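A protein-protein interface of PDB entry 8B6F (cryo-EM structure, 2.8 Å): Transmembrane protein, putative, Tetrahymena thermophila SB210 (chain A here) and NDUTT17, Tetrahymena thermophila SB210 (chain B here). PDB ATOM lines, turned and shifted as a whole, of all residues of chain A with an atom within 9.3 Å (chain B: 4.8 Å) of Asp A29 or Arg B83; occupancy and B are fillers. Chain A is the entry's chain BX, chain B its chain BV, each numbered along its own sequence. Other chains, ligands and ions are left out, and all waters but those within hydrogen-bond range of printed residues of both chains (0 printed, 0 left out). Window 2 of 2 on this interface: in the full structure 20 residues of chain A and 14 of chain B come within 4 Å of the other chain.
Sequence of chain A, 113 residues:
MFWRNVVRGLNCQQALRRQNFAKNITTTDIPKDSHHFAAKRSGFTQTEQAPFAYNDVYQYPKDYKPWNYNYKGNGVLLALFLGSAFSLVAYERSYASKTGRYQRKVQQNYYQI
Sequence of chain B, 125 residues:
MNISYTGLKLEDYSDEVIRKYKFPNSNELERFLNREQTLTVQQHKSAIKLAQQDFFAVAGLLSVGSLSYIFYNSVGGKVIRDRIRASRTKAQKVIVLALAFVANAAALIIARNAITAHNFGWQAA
Printed residues of chain B within 4 Å of Thr A27: Ile B84.
Of chain B, only Arg B83 comes within 4 Å of Asp A29.
Printed residues of chain B within 4 Å of Pro A61: Val B79 (3.7 Å).
Of the printed residues of chain B, Tyr A64 touches Val B79.
No residue of chain A comes within 4 Å of Asp B82.
Arg B83 touches just these residues of chain A: Thr A28 (2.9 Å), Asp A29 (2.7 Å) and Pro A31 (3.3 Å).
Of the printed residues of chain A, Ile B84 touches Thr A27 and Thr A28.
No residue of chain A comes within 4 Å of Ala B86.
The nearest printed residue of chain B that does not touch Thr A27 is Ile B80 (5.1 Å).
Among the printed residues, pairs that only touch across the chains: Thr A27 with Ile B84, Thr A28 with Ile B80, Thr A28 with Ile B84, Pro A31 with Arg B83, Pro A61 with Val B79 and Tyr A64 with Val B79.
The guanidinium group (NH1) of Arg B83 lies within hydrogen-bond range of the side-chain hydroxyl (OG1) of Thr A28.
The side-chain carboxylate (OD1) of Asp A29 is in salt-bridge range of the guanidinium group (NH2) of Arg B83, 2.9 Å away.
Printed residues of chain B that touch a printed residue of chain A: Val B79, Ile B80, Arg B83 and Ile B84.
Along chain B the printed residues that touch a printed residue of chain A span positions 79 to 84.
The backbone carbonyl oxygen of Arg B83 is in hydrogen-bond range of the side-chain hydroxyl of Ser B87 (3.3 Å).
The side-chain hydroxyl (OG) of Ser B87 lies within hydrogen-bond range of the backbone carbonyl oxygen (O) of Ile B84 (2.8 Å).
The side-chain hydroxyl (OG1) of Thr A28 sits at hydrogen-bond distance from the side-chain carboxylate (OD1) of Asp A29.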
ATOM      1  N   LYS A  23     -36.046  22.781 -35.614  1.00  0.00           N
ATOM      2  CA  LYS A  23     -34.813  22.798 -34.834  1.00  0.00           C
ATOM      3  C   LYS A  23     -35.098  22.821 -33.337  1.00  0.00           C
ATOM      4  O   LYS A  23     -34.451  22.103 -32.566  1.00  0.00           O
ATOM      5  CB  LYS A  23     -33.965  24.006 -35.229  1.00  0.00           C
ATOM      6  CG  LYS A  23     -33.370  23.930 -36.627  1.00  0.00           C
ATOM      7  CD  LYS A  23     -32.203  22.957 -36.685  1.00  0.00           C
ATOM      8  CE  LYS A  23     -31.518  23.004 -38.039  1.00  0.00           C
ATOM      9  NZ  LYS A  23     -30.313  22.132 -38.080  1.00  0.00           N
ATOM     10  N   ASN A  24     -36.056  23.638 -32.904  1.00  0.00           N
ATOM     11  CA  ASN A  24     -36.316  23.839 -31.478  1.00  0.00           C
ATOM     12  C   ASN A  24     -37.089  22.643 -30.943  1.00  0.00           C
ATOM     13  O   ASN A  24     -38.319  22.597 -30.980  1.00  0.00           O
ATOM     14  CB  ASN A  24     -37.077  25.138 -31.252  1.00  0.00           C
ATOM     15  CG  ASN A  24     -36.323  26.346 -31.760  1.00  0.00           C
ATOM     16  OD1 ASN A  24     -35.409  26.843 -31.103  1.00  0.00           O
ATOM     17  ND2 ASN A  24     -36.705  26.831 -32.936  1.00  0.00           N
ATOM     18  N   ILE A  25     -36.356  21.664 -30.426  1.00  0.00           N
ATOM     19  CA  ILE A  25     -36.962  20.476 -29.845  1.00  0.00           C
ATOM     20  C   ILE A  25     -37.308  20.750 -28.386  1.00  0.00           C
ATOM     21  O   ILE A  25     -36.744  21.635 -27.740  1.00  0.00           O
ATOM     22  CB  ILE A  25     -36.038  19.248 -29.972  1.00  0.00           C
ATOM     23  CG1 ILE A  25     -34.685  19.521 -29.306  1.00  0.00           C
ATOM     24  CG2 ILE A  25     -35.856  18.881 -31.436  1.00  0.00           C
ATOM     25  CD1 ILE A  25     -33.819  18.292 -29.158  1.00  0.00           C
ATOM     26  N   THR A  26     -38.255  19.972 -27.861  1.00  0.00           N
ATOM     27  CA  THR A  26     -38.689  20.101 -26.478  1.00  0.00           C
ATOM     28  C   THR A  26     -38.288  18.925 -25.601  1.00  0.00           C
ATOM     29  O   THR A  26     -38.472  18.998 -24.382  1.00  0.00           O
ATOM     30  CB  THR A  26     -40.214  20.268 -26.409  1.00  0.00           C
ATOM     31  OG1 THR A  26     -40.848  19.262 -27.209  1.00  0.00           O
ATOM     32  CG2 THR A  26     -40.621  21.638 -26.897  1.00  0.00           C
ATOM     33  N   THR A  27     -37.756  17.848 -26.180  1.00  0.00           N
ATOM     34  CA  THR A  27     -37.332  16.716 -25.365  1.00  0.00           C
ATOM     35  C   THR A  27     -36.238  17.116 -24.387  1.00  0.00           C
ATOM     36  O   THR A  27     -36.175  16.584 -23.274  1.00  0.00           O
ATOM     37  CB  THR A  27     -36.851  15.573 -26.259  1.00  0.00           C
ATOM     38  OG1 THR A  27     -35.803  16.038 -27.118  1.00  0.00           O
ATOM     39  CG2 THR A  27     -37.996  15.038 -27.103  1.00  0.00           C
ATOM     40  N   THR A  28     -35.369  18.044 -24.779  1.00  0.00           N
ATOM     41  CA  THR A  28     -34.314  18.525 -23.901  1.00  0.00           C
ATOM     42  C   THR A  28     -33.874  19.900 -24.378  1.00  0.00           C
ATOM     43  O   THR A  28     -34.175  20.314 -25.499  1.00  0.00           O
ATOM     44  CB  THR A  28     -33.123  17.560 -23.870  1.00  0.00           C
ATOM     45  OG1 THR A  28     -32.117  18.063 -22.983  1.00  0.00           O
ATOM     46  CG2 THR A  28     -32.527  17.387 -25.262  1.00  0.00           C
ATOM     47  N   ASP A  29     -33.154  20.602 -23.506  1.00  0.00           N
ATOM     48  CA  ASP A  29     -32.629  21.922 -23.822  1.00  0.00           C
ATOM     49  C   ASP A  29     -31.260  21.781 -24.473  1.00  0.00           C
ATOM     50  O   ASP A  29     -30.395  21.060 -23.967  1.00  0.00           O
ATOM     51  CB  ASP A  29     -32.536  22.786 -22.564  1.00  0.00           C
ATOM     52  CG  ASP A  29     -31.643  22.178 -21.502  1.00  0.00           C
ATOM     53  OD1 ASP A  29     -31.528  20.936 -21.460  1.00  0.00           O
ATOM     54  OD2 ASP A  29     -31.059  22.942 -20.706  1.00  0.00           O
ATOM     55  N   ILE A  30     -31.072  22.465 -25.593  1.00  0.00           N
ATOM     56  CA  ILE A  30     -29.817  22.354 -26.342  1.00  0.00           C
ATOM     57  C   ILE A  30     -28.679  22.927 -25.504  1.00  0.00           C
ATOM     58  O   ILE A  30     -28.812  24.041 -24.970  1.00  0.00           O
ATOM     59  CB  ILE A  30     -29.930  23.089 -27.681  1.00  0.00           C
ATOM     60  CG1 ILE A  30     -31.134  22.574 -28.477  1.00  0.00           C
ATOM     61  CG2 ILE A  30     -28.648  22.918 -28.487  1.00  0.00           C
ATOM     62  CD1 ILE A  30     -31.390  23.322 -29.771  1.00  0.00           C
ATOM     63  N   PRO A  31     -27.560  22.221 -25.344  1.00  0.00           N
ATOM     64  CA  PRO A  31     -26.390  22.846 -24.716  1.00  0.00           C
ATOM     65  C   PRO A  31     -25.931  24.043 -25.531  1.00  0.00           C
ATOM     66  O   PRO A  31     -25.935  24.013 -26.763  1.00  0.00           O
ATOM     67  CB  PRO A  31     -25.341  21.728 -24.713  1.00  0.00           C
ATOM     68  CG  PRO A  31     -26.105  20.477 -24.865  1.00  0.00           C
ATOM     69  CD  PRO A  31     -27.305  20.813 -25.690  1.00  0.00           C
ATOM     70  N   LYS A  32     -25.523  25.101 -24.839  1.00  0.00           N
ATOM     71  CA  LYS A  32     -25.134  26.315 -25.536  1.00  0.00           C
ATOM     72  C   LYS A  32     -24.217  27.143 -24.652  1.00  0.00           C
ATOM     73  O   LYS A  32     -24.213  27.013 -23.426  1.00  0.00           O
ATOM     74  CB  LYS A  32     -26.359  27.136 -25.949  1.00  0.00           C
ATOM     75  CG  LYS A  32     -27.208  27.601 -24.779  1.00  0.00           C
ATOM     76  CD  LYS A  32     -28.357  28.478 -25.243  1.00  0.00           C
ATOM     77  CE  LYS A  32     -29.161  29.006 -24.064  1.00  0.00           C
ATOM     78  NZ  LYS A  32     -28.335  29.824 -23.131  1.00  0.00           N
ATOM     79  N   TYR A  58     -22.814  26.200 -30.000  1.00  0.00           N
ATOM     80  CA  TYR A  58     -22.911  24.871 -29.415  1.00  0.00           C
ATOM     81  C   TYR A  58     -21.762  24.636 -28.444  1.00  0.00           C
ATOM     82  O   TYR A  58     -20.615  25.000 -28.716  1.00  0.00           O
ATOM     83  CB  TYR A  58     -22.895  23.802 -30.508  1.00  0.00           C
ATOM     84  CG  TYR A  58     -24.153  23.755 -31.342  1.00  0.00           C
ATOM     85  CD1 TYR A  58     -25.290  23.108 -30.881  1.00  0.00           C
ATOM     86  CD2 TYR A  58     -24.200  24.350 -32.594  1.00  0.00           C
ATOM     87  CE1 TYR A  58     -26.443  23.060 -31.641  1.00  0.00           C
ATOM     88  CE2 TYR A  58     -25.346  24.308 -33.362  1.00  0.00           C
ATOM     89  CZ  TYR A  58     -26.464  23.661 -32.881  1.00  0.00           C
ATOM     90  OH  TYR A  58     -27.607  23.619 -33.643  1.00  0.00           O
ATOM     91  N   GLN A  59     -22.075  24.030 -27.304  1.00  0.00           N
ATOM     92  CA  GLN A  59     -21.078  23.666 -26.307  1.00  0.00           C
ATOM     93  C   GLN A  59     -21.140  22.162 -26.093  1.00  0.00           C
ATOM     94  O   GLN A  59     -22.182  21.632 -25.693  1.00  0.00           O
ATOM     95  CB  GLN A  59     -21.308  24.407 -24.990  1.00  0.00           C
ATOM     96  CG  GLN A  59     -20.204  24.188 -23.971  1.00  0.00           C
ATOM     97  CD  GLN A  59     -20.440  24.953 -22.690  1.00  0.00           C
ATOM     98  OE1 GLN A  59     -21.540  25.443 -22.439  1.00  0.00           O
ATOM     99  NE2 GLN A  59     -19.402  25.066 -21.870  1.00  0.00           N
ATOM    100  N   TYR A  60     -20.035  21.485 -26.353  1.00  0.00           N
ATOM    101  CA  TYR A  60     -19.982  20.046 -26.180  1.00  0.00           C
ATOM    102  C   TYR A  60     -19.656  19.692 -24.733  1.00  0.00           C
ATOM    103  O   TYR A  60     -18.990  20.459 -24.033  1.00  0.00           O
ATOM    104  CB  TYR A  60     -18.932  19.439 -27.103  1.00  0.00           C
ATOM    105  CG  TYR A  60     -19.342  19.404 -28.552  1.00  0.00           C
ATOM    106  CD1 TYR A  60     -19.483  20.575 -29.282  1.00  0.00           C
ATOM    107  CD2 TYR A  60     -19.582  18.199 -29.194  1.00  0.00           C
ATOM    108  CE1 TYR A  60     -19.857  20.547 -30.608  1.00  0.00           C
ATOM    109  CE2 TYR A  60     -19.956  18.159 -30.519  1.00  0.00           C
ATOM    110  CZ  TYR A  60     -20.091  19.336 -31.221  1.00  0.00           C
ATOM    111  OH  TYR A  60     -20.461  19.305 -32.544  1.00  0.00           O
ATOM    112  N   PRO A  61     -20.115  18.537 -24.258  1.00  0.00           N
ATOM    113  CA  PRO A  61     -19.744  18.113 -22.905  1.00  0.00           C
ATOM    114  C   PRO A  61     -18.259  17.806 -22.828  1.00  0.00           C
ATOM    115  O   PRO A  61     -17.695  17.157 -23.712  1.00  0.00           O
ATOM    116  CB  PRO A  61     -20.592  16.857 -22.678  1.00  0.00           C
ATOM    117  CG  PRO A  61     -20.867  16.341 -24.039  1.00  0.00           C
ATOM    118  CD  PRO A  61     -20.965  17.542 -24.933  1.00  0.00           C
ATOM    119  N   LYS A  62     -17.627  18.280 -21.761  1.00  0.00           N
ATOM    120  CA  LYS A  62     -16.214  17.998 -21.564  1.00  0.00           C
ATOM    121  C   LYS A  62     -15.999  16.495 -21.442  1.00  0.00           C
ATOM    122  O   LYS A  62     -16.840  15.766 -20.909  1.00  0.00           O
ATOM    123  CB  LYS A  62     -15.694  18.714 -20.317  1.00  0.00           C
ATOM    124  CG  LYS A  62     -15.842  20.230 -20.362  1.00  0.00           C
ATOM    125  CD  LYS A  62     -14.990  20.848 -21.464  1.00  0.00           C
ATOM    126  CE  LYS A  62     -15.164  22.360 -21.526  1.00  0.00           C
ATOM    127  NZ  LYS A  62     -16.549  22.758 -21.900  1.00  0.00           N
ATOM    128  N   TYR A  64     -15.852  14.647 -24.082  1.00  0.00           N
ATOM    129  CA  TYR A  64     -16.424  14.045 -25.278  1.00  0.00           C
ATOM    130  C   TYR A  64     -15.345  13.904 -26.342  1.00  0.00           C
ATOM    131  O   TYR A  64     -14.683  14.882 -26.701  1.00  0.00           O
ATOM    132  CB  TYR A  64     -17.584  14.889 -25.806  1.00  0.00           C
ATOM    133  CG  TYR A  64     -18.170  14.366 -27.098  1.00  0.00           C
ATOM    134  CD1 TYR A  64     -19.162  13.397 -27.088  1.00  0.00           C
ATOM    135  CD2 TYR A  64     -17.730  14.842 -28.326  1.00  0.00           C
ATOM    136  CE1 TYR A  64     -19.700  12.915 -28.265  1.00  0.00           C
ATOM    137  CE2 TYR A  64     -18.262  14.367 -29.508  1.00  0.00           C
ATOM    138  CZ  TYR A  64     -19.246  13.404 -29.471  1.00  0.00           C
ATOM    139  OH  TYR A  64     -19.777  12.926 -30.645  1.00  0.00           O
ATOM    140  N   VAL B  79     -24.731  13.475 -28.495  1.00  0.00           N
ATOM    141  CA  VAL B  79     -24.785  14.345 -27.326  1.00  0.00           C
ATOM    142  C   VAL B  79     -26.223  14.509 -26.856  1.00  0.00           C
ATOM    143  O   VAL B  79     -26.515  14.432 -25.657  1.00  0.00           O
ATOM    144  CB  VAL B  79     -24.134  15.706 -27.639  1.00  0.00           C
ATOM    145  CG1 VAL B  79     -24.219  16.633 -26.433  1.00  0.00           C
ATOM    146  CG2 VAL B  79     -22.688  15.519 -28.067  1.00  0.00           C
ATOM    147  N   ILE B  80     -27.145  14.741 -27.791  1.00  0.00           N
ATOM    148  CA  ILE B  80     -28.543  14.954 -27.426  1.00  0.00           C
ATOM    149  C   ILE B  80     -29.115  13.705 -26.768  1.00  0.00           C
ATOM    150  O   ILE B  80     -29.792  13.779 -25.737  1.00  0.00           O
ATOM    151  CB  ILE B  80     -29.361  15.367 -28.665  1.00  0.00           C
ATOM    152  CG1 ILE B  80     -28.734  16.589 -29.345  1.00  0.00           C
ATOM    153  CG2 ILE B  80     -30.806  15.653 -28.285  1.00  0.00           C
ATOM    154  CD1 ILE B  80     -28.544  17.789 -28.438  1.00  0.00           C
ATOM    155  N   ARG B  81     -28.848  12.536 -27.354  1.00  0.00           N
ATOM    156  CA  ARG B  81     -29.357  11.291 -26.786  1.00  0.00           C
ATOM    157  C   ARG B  81     -28.787  11.043 -25.399  1.00  0.00           C
ATOM    158  O   ARG B  81     -29.510  10.626 -24.487  1.00  0.00           O
ATOM    159  CB  ARG B  81     -29.031  10.118 -27.709  1.00  0.00           C
ATOM    160  CG  ARG B  81     -29.793  10.134 -29.020  1.00  0.00           C
ATOM    161  CD  ARG B  81     -29.409   8.953 -29.886  1.00  0.00           C
ATOM    162  NE  ARG B  81     -27.998   8.983 -30.248  1.00  0.00           N
ATOM    163  CZ  ARG B  81     -27.393   8.056 -30.979  1.00  0.00           C
ATOM    164  NH1 ARG B  81     -28.047   7.004 -31.440  1.00  0.00           N
ATOM    165  NH2 ARG B  81     -26.100   8.192 -31.257  1.00  0.00           N
ATOM    166  N   ASP B  82     -27.489  11.286 -25.219  1.00  0.00           N
ATOM    167  CA  ASP B  82     -26.872  11.067 -23.916  1.00  0.00           C
ATOM    168  C   ASP B  82     -27.472  11.989 -22.862  1.00  0.00           C
ATOM    169  O   ASP B  82     -27.743  11.559 -21.734  1.00  0.00           O
ATOM    170  CB  ASP B  82     -25.361  11.275 -24.017  1.00  0.00           C
ATOM    171  CG  ASP B  82     -24.614  10.705 -22.828  1.00  0.00           C
ATOM    172  OD1 ASP B  82     -25.204  10.635 -21.729  1.00  0.00           O
ATOM    173  OD2 ASP B  82     -23.435  10.327 -22.990  1.00  0.00           O
ATOM    174  N   ARG B  83     -27.684  13.262 -23.204  1.00  0.00           N
ATOM    175  CA  ARG B  83     -28.266  14.193 -22.240  1.00  0.00           C
ATOM    176  C   ARG B  83     -29.705  13.820 -21.907  1.00  0.00           C
ATOM    177  O   ARG B  83     -30.121  13.907 -20.747  1.00  0.00           O
ATOM    178  CB  ARG B  83     -28.189  15.622 -22.777  1.00  0.00           C
ATOM    179  CG  ARG B  83     -26.766  16.134 -22.903  1.00  0.00           C
ATOM    180  CD  ARG B  83     -26.708  17.573 -23.380  1.00  0.00           C
ATOM    181  NE  ARG B  83     -27.239  18.506 -22.392  1.00  0.00           N
ATOM    182  CZ  ARG B  83     -28.463  19.016 -22.410  1.00  0.00           C
ATOM    183  NH1 ARG B  83     -29.335  18.699 -23.355  1.00  0.00           N
ATOM    184  NH2 ARG B  83     -28.824  19.867 -21.454  1.00  0.00           N
ATOM    185  N   ILE B  84     -30.483  13.410 -22.910  1.00  0.00           N
ATOM    186  CA  ILE B  84     -31.863  13.007 -22.656  1.00  0.00           C
ATOM    187  C   ILE B  84     -31.901  11.796 -21.736  1.00  0.00           C
ATOM    188  O   ILE B  84     -32.696  11.740 -20.789  1.00  0.00           O
ATOM    189  CB  ILE B  84     -32.597  12.744 -23.984  1.00  0.00           C
ATOM    190  CG1 ILE B  84     -32.827  14.072 -24.704  1.00  0.00           C
ATOM    191  CG2 ILE B  84     -33.918  12.012 -23.744  1.00  0.00           C
ATOM    192  CD1 ILE B  84     -33.382  13.940 -26.083  1.00  0.00           C
ATOM    193  N   ARG B  85     -31.049  10.805 -21.998  1.00  0.00           N
ATOM    194  CA  ARG B  85     -31.021   9.619 -21.152  1.00  0.00           C
ATOM    195  C   ARG B  85     -30.515   9.944 -19.753  1.00  0.00           C
ATOM    196  O   ARG B  85     -30.962   9.330 -18.779  1.00  0.00           O
ATOM    197  CB  ARG B  85     -30.157   8.533 -21.796  1.00  0.00           C
ATOM    198  CG  ARG B  85     -30.201   7.205 -21.058  1.00  0.00           C
ATOM    199  CD  ARG B  85     -29.802   6.042 -21.954  1.00  0.00           C
ATOM    200  NE  ARG B  85     -30.736   5.857 -23.058  1.00  0.00           N
ATOM    201  CZ  ARG B  85     -30.729   4.820 -23.884  1.00  0.00           C
ATOM    202  NH1 ARG B  85     -29.853   3.837 -23.754  1.00  0.00           N
ATOM    203  NH2 ARG B  85     -31.625   4.766 -24.865  1.00  0.00           N
ATOM    204  N   ALA B  86     -29.589  10.896 -19.629  1.00  0.00           N
ATOM    205  CA  ALA B  86     -29.136  11.300 -18.303  1.00  0.00           C
ATOM    206  C   ALA B  86     -30.266  11.942 -17.507  1.00  0.00           C
ATOM    207  O   ALA B  86     -30.449  11.638 -16.322  1.00  0.00           O
ATOM    208  CB  ALA B  86     -27.955  12.264 -18.427  1.00  0.00           C
ATOM    209  N   SER B  87     -31.032  12.835 -18.136  1.00  0.00           N
ATOM    210  CA  SER B  87     -32.190  13.422 -17.471  1.00  0.00           C
ATOM    211  C   SER B  87     -33.300  12.402 -17.259  1.00  0.00           C
ATOM    212  O   SER B  87     -34.196  12.636 -16.442  1.00  0.00           O
ATOM    213  CB  SER B  87     -32.719  14.607 -18.278  1.00  0.00           C
ATOM    214  OG  SER B  87     -33.200  14.192 -19.545  1.00  0.00           O
